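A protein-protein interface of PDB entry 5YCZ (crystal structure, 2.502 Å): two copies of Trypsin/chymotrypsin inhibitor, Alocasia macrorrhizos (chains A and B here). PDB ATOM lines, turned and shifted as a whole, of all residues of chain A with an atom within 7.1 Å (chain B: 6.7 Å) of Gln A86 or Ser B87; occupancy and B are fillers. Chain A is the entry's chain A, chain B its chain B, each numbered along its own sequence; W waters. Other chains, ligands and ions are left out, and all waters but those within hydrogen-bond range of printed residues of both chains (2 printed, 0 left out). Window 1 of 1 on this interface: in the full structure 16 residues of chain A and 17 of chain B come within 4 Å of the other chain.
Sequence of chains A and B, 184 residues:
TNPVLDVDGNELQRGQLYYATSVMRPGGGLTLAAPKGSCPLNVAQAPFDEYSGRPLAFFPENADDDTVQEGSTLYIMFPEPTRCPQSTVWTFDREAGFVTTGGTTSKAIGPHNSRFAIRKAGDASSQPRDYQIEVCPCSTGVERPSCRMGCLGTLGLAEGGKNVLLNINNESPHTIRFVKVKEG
Cys A84 touches Gly B103, and with the chains exchanged Gly A103 touches Cys B84.
Pro A85 touches Gln B86, and with the chains exchanged Gln A86 touches Pro B85.
Pro A85 touches Ser B87, and with the chains exchanged Ser A87 touches Pro B85.
Gln A86 touches Ser B87, and with the chains exchanged Ser A87 touches Gln B86.
Positions printed for both chains: 40, 41, 84, 85, 86, 87, 88, 89, 101, 102 and 103.
Of the 18 pairs that touch across the chains among the printed residues, 11 have their exchanged pair printed and touching as well.
The backbone NH of Gly B102 sits at hydrogen-bond distance from the backbone carbonyl oxygen of Val B89 (3.3 Å).
The side-chain hydroxyl of Ser A87 is in hydrogen-bond range of the backbone carbonyl oxygen of Gly A103 (2.8 Å).
The side-chain hydroxyl (OG) of Ser B87 sits at hydrogen-bond distance from the backbone carbonyl oxygen (O) of Gly B103 (3.0 Å).
The backbone carbonyl oxygen of Val B89 lies within hydrogen-bond range of the backbone NH of Gly B103 (2.9 Å).
The guanidinium group (NH1) of Arg A83 lies within hydrogen-bond range of the side-chain sulfur (SG) of Cys A84 (3.8 Å).
The side-chain hydroxyl (OG) of Ser B87 sits close to the backbone NH (N) of Val B89 (3.3 Å).
Along chain A the printed residues that touch a printed residue of chain B span positions 80 to 103.
Hydrophobic or aromatic side chains of chain B within 4 Å of the printed part of chain A: Met B77 and Val B89.
Among the printed residues, 18 pairs touch across the chains.
N of Ser B87 is in hydrogen-bond range of O of Pro A85 (2.7 Å).
The backbone NH (N) of Ser A87 lies within hydrogen-bond range of the backbone carbonyl oxygen (O) of Pro B85 (2.7 Å).
The backbone carbonyl oxygen (O) of Glu A80 lies close to the side-chain sulfur (SD) of Met B77 (3.7 Å).
N of Pro A81 sits close to SD of Met B77 (3.7 Å).
The backbone NH (N) of Ser A87 sits close to the backbone NH (N) of Ser B87, at 3.2 Å.
Ser B87 touches just these residues of chain A: Pro A85, Gln A86 and Ser A87.
Of the printed residues of chain A, Gly B102 touches Pro A85.
Of the printed residues of chain A, Cys B84 touches Gly A103 (3.97 Å).
Of the printed residues of chain B, Arg A83 touches Thr B104 (3.5 Å).
Printed residues of chain B within 4 Å of Gly A103: Cys B84 (3.97 Å).
Phe B78 touches none of the printed residues of chain A.
Thr A82 touches Thr B104 (O to CA, 3.1 Å).
Arg A83 touches Thr B104.
Cys A84 touches Gly B103 (O to O, 3.9 Å).
CG2 of Thr B104 touches C of Cys A84, at 3.3 Å.
Pro A85 touches Gly B102 (CB to O, 3.6 Å).
O of Pro B85 touches CA of Gln A86, 3.4 Å away.
Ser B87 touches Gln A86 (CB to O, 3.4 Å).
Gln B86 touches Ser A87 (C to N, 3.4 Å).
Gly A102 touches Pro B85.
Cys B84 touches Gly A103.
Water W2 lies within hydrogen-bond range of the backbone carbonyl oxygen of Gly A103 (2.9 Å), the backbone carbonyl oxygen of Cys B84 (2.9 Å) and the side-chain hydroxyl of Ser A87 (3.3 Å).
Water W1 lies within hydrogen-bond range of N of Thr A82 (3.1 Å), O of Gly B103 (3.1 Å), O of Cys A84 (3.3 Å) and OG of Ser B87 (3.3 Å).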
ATOM      1  N   SER A  38      -3.967 -12.203   4.402  1.00  0.00           N
ATOM      2  CA  SER A  38      -4.038 -13.646   4.250  1.00  0.00           C
ATOM      3  C   SER A  38      -4.328 -14.262   5.611  1.00  0.00           C
ATOM      4  O   SER A  38      -3.782 -13.816   6.624  1.00  0.00           O
ATOM      5  CB  SER A  38      -2.720 -14.189   3.681  1.00  0.00           C
ATOM      6  OG  SER A  38      -2.913 -15.415   2.998  1.00  0.00           O
ATOM      7  N   CYS A  39      -5.193 -15.274   5.642  1.00  0.00           N
ATOM      8  CA  CYS A  39      -5.379 -16.038   6.868  1.00  0.00           C
ATOM      9  C   CYS A  39      -5.397 -17.514   6.515  1.00  0.00           C
ATOM     10  O   CYS A  39      -5.881 -17.880   5.442  1.00  0.00           O
ATOM     11  CB  CYS A  39      -6.677 -15.667   7.606  1.00  0.00           C
ATOM     12  SG  CYS A  39      -6.644 -14.055   8.503  1.00  0.00           S
ATOM     13  N   PRO A  40      -4.867 -18.393   7.395  1.00  0.00           N
ATOM     14  CA  PRO A  40      -4.331 -18.076   8.725  1.00  0.00           C
ATOM     15  C   PRO A  40      -2.864 -17.670   8.690  1.00  0.00           C
ATOM     16  O   PRO A  40      -2.211 -17.852   7.668  1.00  0.00           O
ATOM     17  CB  PRO A  40      -4.500 -19.397   9.504  1.00  0.00           C
ATOM     18  CG  PRO A  40      -4.874 -20.436   8.493  1.00  0.00           C
ATOM     19  CD  PRO A  40      -4.748 -19.831   7.118  1.00  0.00           C
ATOM     20  N   LEU A  41      -2.380 -17.099   9.791  1.00  0.00           N
ATOM     21  CA  LEU A  41      -0.955 -16.875   9.959  1.00  0.00           C
ATOM     22  C   LEU A  41      -0.242 -18.208  10.126  1.00  0.00           C
ATOM     23  O   LEU A  41      -0.810 -19.176  10.647  1.00  0.00           O
ATOM     24  CB  LEU A  41      -0.690 -15.988  11.174  1.00  0.00           C
ATOM     25  CG  LEU A  41      -1.633 -14.791  11.317  1.00  0.00           C
ATOM     26  CD1 LEU A  41      -1.197 -13.964  12.493  1.00  0.00           C
ATOM     27  CD2 LEU A  41      -1.614 -13.949  10.056  1.00  0.00           C
ATOM     28  N   GLU A  80      -1.324 -14.132  22.229  1.00  0.00           N
ATOM     29  CA  GLU A  80      -1.656 -12.746  21.946  1.00  0.00           C
ATOM     30  C   GLU A  80      -2.781 -12.722  20.931  1.00  0.00           C
ATOM     31  O   GLU A  80      -3.039 -13.724  20.255  1.00  0.00           O
ATOM     32  CB  GLU A  80      -0.452 -11.942  21.428  1.00  0.00           C
ATOM     33  CG  GLU A  80       0.437 -12.672  20.470  1.00  0.00           C
ATOM     34  CD  GLU A  80       1.677 -11.862  20.132  1.00  0.00           C
ATOM     35  OE1 GLU A  80       1.607 -11.026  19.198  1.00  0.00           O
ATOM     36  OE2 GLU A  80       2.720 -12.046  20.815  1.00  0.00           O
ATOM     37  N   PRO A  81      -3.496 -11.613  20.823  1.00  0.00           N
ATOM     38  CA  PRO A  81      -4.478 -11.504  19.760  1.00  0.00           C
ATOM     39  C   PRO A  81      -3.753 -11.297  18.450  1.00  0.00           C
ATOM     40  O   PRO A  81      -2.554 -10.996  18.382  1.00  0.00           O
ATOM     41  CB  PRO A  81      -5.331 -10.290  20.143  1.00  0.00           C
ATOM     42  CG  PRO A  81      -4.979 -10.002  21.544  1.00  0.00           C
ATOM     43  CD  PRO A  81      -3.543 -10.430  21.695  1.00  0.00           C
ATOM     44  N   THR A  82      -4.546 -11.416  17.401  1.00  0.00           N
ATOM     45  CA  THR A  82      -4.047 -11.620  16.066  1.00  0.00           C
ATOM     46  C   THR A  82      -5.086 -11.038  15.135  1.00  0.00           C
ATOM     47  O   THR A  82      -6.253 -10.891  15.508  1.00  0.00           O
ATOM     48  CB  THR A  82      -3.815 -13.118  15.865  1.00  0.00           C
ATOM     49  OG1 THR A  82      -2.564 -13.490  16.457  1.00  0.00           O
ATOM     50  CG2 THR A  82      -3.877 -13.538  14.440  1.00  0.00           C
ATOM     51  N   ARG A  83      -4.650 -10.684  13.931  1.00  0.00           N
ATOM     52  CA  ARG A  83      -5.563 -10.204  12.905  1.00  0.00           C
ATOM     53  C   ARG A  83      -6.410 -11.305  12.272  1.00  0.00           C
ATOM     54  O   ARG A  83      -7.287 -10.996  11.454  1.00  0.00           O
ATOM     55  CB  ARG A  83      -4.773  -9.475  11.808  1.00  0.00           C
ATOM     56  CG  ARG A  83      -3.869 -10.366  10.967  1.00  0.00           C
ATOM     57  CD  ARG A  83      -3.522  -9.638   9.681  1.00  0.00           C
ATOM     58  NE  ARG A  83      -2.329 -10.137   9.011  1.00  0.00           N
ATOM     59  CZ  ARG A  83      -2.357 -11.030   8.036  1.00  0.00           C
ATOM     60  NH1 ARG A  83      -3.528 -11.522   7.646  1.00  0.00           N
ATOM     61  NH2 ARG A  83      -1.217 -11.426   7.465  1.00  0.00           N
ATOM     62  N   CYS A  84      -6.166 -12.567  12.604  1.00  0.00           N
ATOM     63  CA  CYS A  84      -6.890 -13.702  12.061  1.00  0.00           C
ATOM     64  C   CYS A  84      -7.675 -14.383  13.170  1.00  0.00           C
ATOM     65  O   CYS A  84      -7.299 -14.312  14.344  1.00  0.00           O
ATOM     66  CB  CYS A  84      -5.954 -14.723  11.408  1.00  0.00           C
ATOM     67  SG  CYS A  84      -5.115 -14.141   9.890  1.00  0.00           S
ATOM     68  N   PRO A  85      -8.791 -15.027  12.830  1.00  0.00           N
ATOM     69  CA  PRO A  85      -9.699 -15.553  13.854  1.00  0.00           C
ATOM     70  C   PRO A  85      -9.338 -16.928  14.387  1.00  0.00           C
ATOM     71  O   PRO A  85      -9.932 -17.355  15.398  1.00  0.00           O
ATOM     72  CB  PRO A  85     -11.019 -15.616  13.095  1.00  0.00           C
ATOM     73  CG  PRO A  85     -10.576 -16.011  11.705  1.00  0.00           C
ATOM     74  CD  PRO A  85      -9.358 -15.170  11.477  1.00  0.00           C
ATOM     75  N   GLN A  86      -8.425 -17.632  13.707  1.00  0.00           N
ATOM     76  CA  GLN A  86      -7.961 -18.942  14.144  1.00  0.00           C
ATOM     77  C   GLN A  86      -7.167 -18.813  15.433  1.00  0.00           C
ATOM     78  O   GLN A  86      -6.531 -17.788  15.696  1.00  0.00           O
ATOM     79  CB  GLN A  86      -7.077 -19.592  13.069  1.00  0.00           C
ATOM     80  CG  GLN A  86      -7.771 -19.803  11.743  1.00  0.00           C
ATOM     81  CD  GLN A  86      -7.697 -18.582  10.838  1.00  0.00           C
ATOM     82  OE1 GLN A  86      -6.834 -17.710  11.001  1.00  0.00           O
ATOM     83  NE2 GLN A  86      -8.590 -18.517   9.874  1.00  0.00           N
ATOM     84  N   SER A  87      -7.190 -19.875  16.235  1.00  0.00           N
ATOM     85  CA  SER A  87      -6.354 -19.895  17.428  1.00  0.00           C
ATOM     86  C   SER A  87      -4.892 -19.755  17.039  1.00  0.00           C
ATOM     87  O   SER A  87      -4.477 -20.136  15.945  1.00  0.00           O
ATOM     88  CB  SER A  87      -6.579 -21.178  18.233  1.00  0.00           C
ATOM     89  OG  SER A  87      -6.016 -22.315  17.605  1.00  0.00           O
ATOM     90  N   THR A  88      -4.122 -19.165  17.930  1.00  0.00           N
ATOM     91  CA  THR A  88      -2.681 -19.087  17.777  1.00  0.00           C
ATOM     92  C   THR A  88      -1.962 -20.332  18.306  1.00  0.00           C
ATOM     93  O   THR A  88      -0.766 -20.270  18.617  1.00  0.00           O
ATOM     94  CB  THR A  88      -2.161 -17.843  18.481  1.00  0.00           C
ATOM     95  OG1 THR A  88      -2.684 -17.817  19.816  1.00  0.00           O
ATOM     96  CG2 THR A  88      -2.614 -16.596  17.737  1.00  0.00           C
ATOM     97  N   VAL A  89      -2.677 -21.446  18.445  1.00  0.00           N
ATOM     98  CA  VAL A  89      -2.079 -22.728  18.807  1.00  0.00           C
ATOM     99  C   VAL A  89      -1.412 -23.322  17.573  1.00  0.00           C
ATOM    100  O   VAL A  89      -2.029 -23.415  16.509  1.00  0.00           O
ATOM    101  CB  VAL A  89      -3.146 -23.687  19.363  1.00  0.00           C
ATOM    102  CG1 VAL A  89      -2.613 -25.082  19.443  1.00  0.00           C
ATOM    103  CG2 VAL A  89      -3.593 -23.253  20.729  1.00  0.00           C
ATOM    104  N   THR A 101      -1.586 -22.149  12.215  1.00  0.00           N
ATOM    105  CA  THR A 101      -2.311 -21.870  13.439  1.00  0.00           C
ATOM    106  C   THR A 101      -3.630 -22.622  13.426  1.00  0.00           C
ATOM    107  O   THR A 101      -3.861 -23.489  12.575  1.00  0.00           O
ATOM    108  CB  THR A 101      -2.487 -20.357  13.598  1.00  0.00           C
ATOM    109  OG1 THR A 101      -2.827 -19.781  12.331  1.00  0.00           O
ATOM    110  CG2 THR A 101      -1.173 -19.735  14.071  1.00  0.00           C
ATOM    111  N   GLY A 102      -4.506 -22.281  14.368  1.00  0.00           N
ATOM    112  CA  GLY A 102      -5.769 -22.984  14.472  1.00  0.00           C
ATOM    113  C   GLY A 102      -5.605 -24.371  15.048  1.00  0.00           C
ATOM    114  O   GLY A 102      -6.165 -25.338  14.517  1.00  0.00           O
ATOM    115  N   GLY A 103      -4.846 -24.495  16.084  1.00  0.00           N
ATOM    116  CA  GLY A 103      -4.658 -25.786  16.682  1.00  0.00           C
ATOM    117  C   GLY A 103      -5.562 -25.992  17.867  1.00  0.00           C
ATOM    118  O   GLY A 103      -6.121 -25.040  18.420  1.00  0.00           O
ATOM    119  N   LEU B  32     -14.639 -20.549  29.300  1.00  0.00           N
ATOM    120  CA  LEU B  32     -15.250 -20.855  28.021  1.00  0.00           C
ATOM    121  C   LEU B  32     -16.023 -22.148  28.157  1.00  0.00           C
ATOM    122  O   LEU B  32     -15.544 -23.104  28.774  1.00  0.00           O
ATOM    123  CB  LEU B  32     -14.217 -21.004  26.906  1.00  0.00           C
ATOM    124  CG  LEU B  32     -13.472 -19.720  26.560  1.00  0.00           C
ATOM    125  CD1 LEU B  32     -12.363 -20.003  25.578  1.00  0.00           C
ATOM    126  CD2 LEU B  32     -14.415 -18.685  25.998  1.00  0.00           C
ATOM    127  N   PRO B  40     -17.845 -22.276  18.036  1.00  0.00           N
ATOM    128  CA  PRO B  40     -16.812 -21.862  18.988  1.00  0.00           C
ATOM    129  C   PRO B  40     -17.333 -21.835  20.396  1.00  0.00           C
ATOM    130  O   PRO B  40     -18.529 -21.999  20.623  1.00  0.00           O
ATOM    131  CB  PRO B  40     -16.442 -20.443  18.529  1.00  0.00           C
ATOM    132  CG  PRO B  40     -17.666 -19.932  17.878  1.00  0.00           C
ATOM    133  CD  PRO B  40     -18.358 -21.132  17.260  1.00  0.00           C
ATOM    134  N   LEU B  41     -16.441 -21.624  21.345  1.00  0.00           N
ATOM    135  CA  LEU B  41     -16.889 -21.544  22.709  1.00  0.00           C
ATOM    136  C   LEU B  41     -17.343 -20.127  23.006  1.00  0.00           C
ATOM    137  O   LEU B  41     -16.924 -19.163  22.352  1.00  0.00           O
ATOM    138  CB  LEU B  41     -15.781 -21.976  23.648  1.00  0.00           C
ATOM    139  CG  LEU B  41     -15.484 -23.454  23.448  1.00  0.00           C
ATOM    140  CD1 LEU B  41     -14.011 -23.623  23.377  1.00  0.00           C
ATOM    141  CD2 LEU B  41     -16.053 -24.288  24.584  1.00  0.00           C
ATOM    142  N   MET B  77      -8.741 -11.860  25.871  1.00  0.00           N
ATOM    143  CA  MET B  77      -8.666 -13.255  25.457  1.00  0.00           C
ATOM    144  C   MET B  77      -8.321 -14.147  26.644  1.00  0.00           C
ATOM    145  O   MET B  77      -7.864 -13.685  27.694  1.00  0.00           O
ATOM    146  CB  MET B  77      -7.653 -13.437  24.316  1.00  0.00           C
ATOM    147  CG  MET B  77      -6.201 -13.462  24.753  1.00  0.00           C
ATOM    148  SD  MET B  77      -4.978 -13.830  23.442  1.00  0.00           S
ATOM    149  CE  MET B  77      -5.658 -15.295  22.660  1.00  0.00           C
ATOM    150  N   PHE B  78      -8.556 -15.447  26.456  1.00  0.00           N
ATOM    151  CA  PHE B  78      -8.092 -16.507  27.347  1.00  0.00           C
ATOM    152  C   PHE B  78      -6.843 -17.154  26.761  1.00  0.00           C
ATOM    153  O   PHE B  78      -6.943 -18.086  25.952  1.00  0.00           O
ATOM    154  CB  PHE B  78      -9.163 -17.576  27.526  1.00  0.00           C
ATOM    155  CG  PHE B  78     -10.377 -17.117  28.256  1.00  0.00           C
ATOM    156  CD1 PHE B  78     -10.329 -16.858  29.616  1.00  0.00           C
ATOM    157  CD2 PHE B  78     -11.587 -17.003  27.596  1.00  0.00           C
ATOM    158  CE1 PHE B  78     -11.468 -16.469  30.298  1.00  0.00           C
ATOM    159  CE2 PHE B  78     -12.725 -16.613  28.263  1.00  0.00           C
ATOM    160  CZ  PHE B  78     -12.669 -16.343  29.618  1.00  0.00           C
ATOM    161  N   CYS B  84     -11.248 -26.065  20.537  1.00  0.00           N
ATOM    162  CA  CYS B  84     -11.835 -25.363  19.390  1.00  0.00           C
ATOM    163  C   CYS B  84     -10.780 -24.585  18.616  1.00  0.00           C
ATOM    164  O   CYS B  84      -9.870 -24.010  19.218  1.00  0.00           O
ATOM    165  CB  CYS B  84     -12.939 -24.384  19.816  1.00  0.00           C
ATOM    166  SG  CYS B  84     -14.467 -25.181  20.270  1.00  0.00           S
ATOM    167  N   PRO B  85     -10.903 -24.536  17.285  1.00  0.00           N
ATOM    168  CA  PRO B  85      -9.883 -23.899  16.445  1.00  0.00           C
ATOM    169  C   PRO B  85      -9.953 -22.388  16.366  1.00  0.00           C
ATOM    170  O   PRO B  85      -9.091 -21.788  15.717  1.00  0.00           O
ATOM    171  CB  PRO B  85     -10.152 -24.521  15.075  1.00  0.00           C
ATOM    172  CG  PRO B  85     -11.574 -24.886  15.109  1.00  0.00           C
ATOM    173  CD  PRO B  85     -11.854 -25.327  16.489  1.00  0.00           C
ATOM    174  N   GLN B  86     -10.920 -21.748  17.007  1.00  0.00           N
ATOM    175  CA  GLN B  86     -10.995 -20.298  17.000  1.00  0.00           C
ATOM    176  C   GLN B  86     -10.086 -19.704  18.067  1.00  0.00           C
ATOM    177  O   GLN B  86      -9.847 -20.306  19.115  1.00  0.00           O
ATOM    178  CB  GLN B  86     -12.432 -19.843  17.256  1.00  0.00           C
ATOM    179  CG  GLN B  86     -13.391 -20.191  16.134  1.00  0.00           C
ATOM    180  CD  GLN B  86     -13.938 -21.590  16.251  1.00  0.00           C
ATOM    181  OE1 GLN B  86     -13.925 -22.187  17.328  1.00  0.00           O
ATOM    182  NE2 GLN B  86     -14.411 -22.134  15.140  1.00  0.00           N
ATOM    183  N   SER B  87      -9.594 -18.499  17.812  1.00  0.00           N
ATOM    184  CA  SER B  87      -8.821 -17.836  18.848  1.00  0.00           C
ATOM    185  C   SER B  87      -9.703 -17.578  20.055  1.00  0.00           C
ATOM    186  O   SER B  87     -10.929 -17.478  19.955  1.00  0.00           O
ATOM    187  CB  SER B  87      -8.254 -16.514  18.347  1.00  0.00           C
ATOM    188  OG  SER B  87      -9.238 -15.503  18.423  1.00  0.00           O
ATOM    189  N   THR B  88      -9.071 -17.449  21.209  1.00  0.00           N
ATOM    190  CA  THR B  88      -9.818 -17.209  22.428  1.00  0.00           C
ATOM    191  C   THR B  88     -10.077 -15.740  22.648  1.00  0.00           C
ATOM    192  O   THR B  88     -10.467 -15.349  23.747  1.00  0.00           O
ATOM    193  CB  THR B  88      -9.083 -17.793  23.628  1.00  0.00           C
ATOM    194  OG1 THR B  88      -7.680 -17.617  23.444  1.00  0.00           O
ATOM    195  CG2 THR B  88      -9.364 -19.270  23.741  1.00  0.00           C
ATOM    196  N   VAL B  89      -9.859 -14.918  21.627  1.00  0.00           N
ATOM    197  CA  VAL B  89     -10.155 -13.492  21.707  1.00  0.00           C
ATOM    198  C   VAL B  89     -11.664 -13.283  21.741  1.00  0.00           C
ATOM    199  O   VAL B  89     -12.407 -13.848  20.928  1.00  0.00           O
ATOM    200  CB  VAL B  89      -9.518 -12.754  20.519  1.00  0.00           C
ATOM    201  CG1 VAL B  89      -9.640 -11.257  20.713  1.00  0.00           C
ATOM    202  CG2 VAL B  89      -8.077 -13.164  20.367  1.00  0.00           C
ATOM    203  N   TRP B  90     -12.129 -12.467  22.677  1.00  0.00           N
ATOM    204  CA  TRP B  90     -13.560 -12.229  22.784  1.00  0.00           C
ATOM    205  C   TRP B  90     -14.041 -11.441  21.584  1.00  0.00           C
ATOM    206  O   TRP B  90     -13.324 -10.600  21.042  1.00  0.00           O
ATOM    207  CB  TRP B  90     -13.899 -11.423  24.023  1.00  0.00           C
ATOM    208  CG  TRP B  90     -13.669 -12.077  25.302  1.00  0.00           C
ATOM    209  CD1 TRP B  90     -12.922 -13.186  25.546  1.00  0.00           C
ATOM    210  CD2 TRP B  90     -14.189 -11.658  26.555  1.00  0.00           C
ATOM    211  NE1 TRP B  90     -12.945 -13.488  26.887  1.00  0.00           N
ATOM    212  CE2 TRP B  90     -13.719 -12.559  27.528  1.00  0.00           C
ATOM    213  CE3 TRP B  90     -15.011 -10.604  26.953  1.00  0.00           C
ATOM    214  CZ2 TRP B  90     -14.035 -12.434  28.867  1.00  0.00           C
ATOM    215  CZ3 TRP B  90     -15.322 -10.480  28.283  1.00  0.00           C
ATOM    216  CH2 TRP B  90     -14.835 -11.387  29.224  1.00  0.00           C
ATOM    217  N   THR B 100     -18.556 -14.221  22.275  1.00  0.00           N
ATOM    218  CA  THR B 100     -18.110 -15.520  21.796  1.00  0.00           C
ATOM    219  C   THR B 100     -16.601 -15.477  21.574  1.00  0.00           C
ATOM    220  O   THR B 100     -15.933 -14.554  22.048  1.00  0.00           O
ATOM    221  CB  THR B 100     -18.888 -15.924  20.536  1.00  0.00           C
ATOM    222  OG1 THR B 100     -18.602 -17.286  20.192  1.00  0.00           O
ATOM    223  CG2 THR B 100     -18.533 -15.047  19.360  1.00  0.00           C
ATOM    224  N   THR B 101     -16.041 -16.460  20.884  1.00  0.00           N
ATOM    225  CA  THR B 101     -14.608 -16.416  20.633  1.00  0.00           C
ATOM    226  C   THR B 101     -14.345 -16.191  19.145  1.00  0.00           C
ATOM    227  O   THR B 101     -15.270 -15.972  18.352  1.00  0.00           O
ATOM    228  CB  THR B 101     -13.930 -17.685  21.146  1.00  0.00           C
ATOM    229  OG1 THR B 101     -14.581 -18.837  20.600  1.00  0.00           O
ATOM    230  CG2 THR B 101     -13.991 -17.728  22.643  1.00  0.00           C
ATOM    231  N   GLY B 102     -13.072 -16.242  18.767  1.00  0.00           N
ATOM    232  CA  GLY B 102     -12.704 -15.999  17.392  1.00  0.00           C
ATOM    233  C   GLY B 102     -12.565 -14.535  17.057  1.00  0.00           C
ATOM    234  O   GLY B 102     -12.791 -14.147  15.907  1.00  0.00           O
ATOM    235  N   GLY B 103     -12.217 -13.704  18.035  1.00  0.00           N
ATOM    236  CA  GLY B 103     -11.977 -12.303  17.773  1.00  0.00           C
ATOM    237  C   GLY B 103     -10.652 -12.055  17.060  1.00  0.00           C
ATOM    238  O   GLY B 103      -9.784 -12.917  16.945  1.00  0.00           O
ATOM    239  N   THR B 104     -10.498 -10.825  16.579  1.00  0.00           N
ATOM    240  CA  THR B 104      -9.312 -10.418  15.842  1.00  0.00           C
ATOM    241  C   THR B 104      -8.935  -9.000  16.229  1.00  0.00           C
ATOM    242  O   THR B 104      -9.797  -8.198  16.599  1.00  0.00           O
ATOM    243  CB  THR B 104      -9.557 -10.460  14.342  1.00  0.00           C
ATOM    244  OG1 THR B 104     -10.799  -9.796  14.074  1.00  0.00           O
ATOM    245  CG2 THR B 104      -9.684 -11.871  13.885  1.00  0.00           C
HETATM  246  O   HOH W   1      -6.782 -13.500  17.452  1.00  0.00           O
HETATM  247  O   HOH W   2      -7.321 -23.384  20.473  1.00  0.00           O
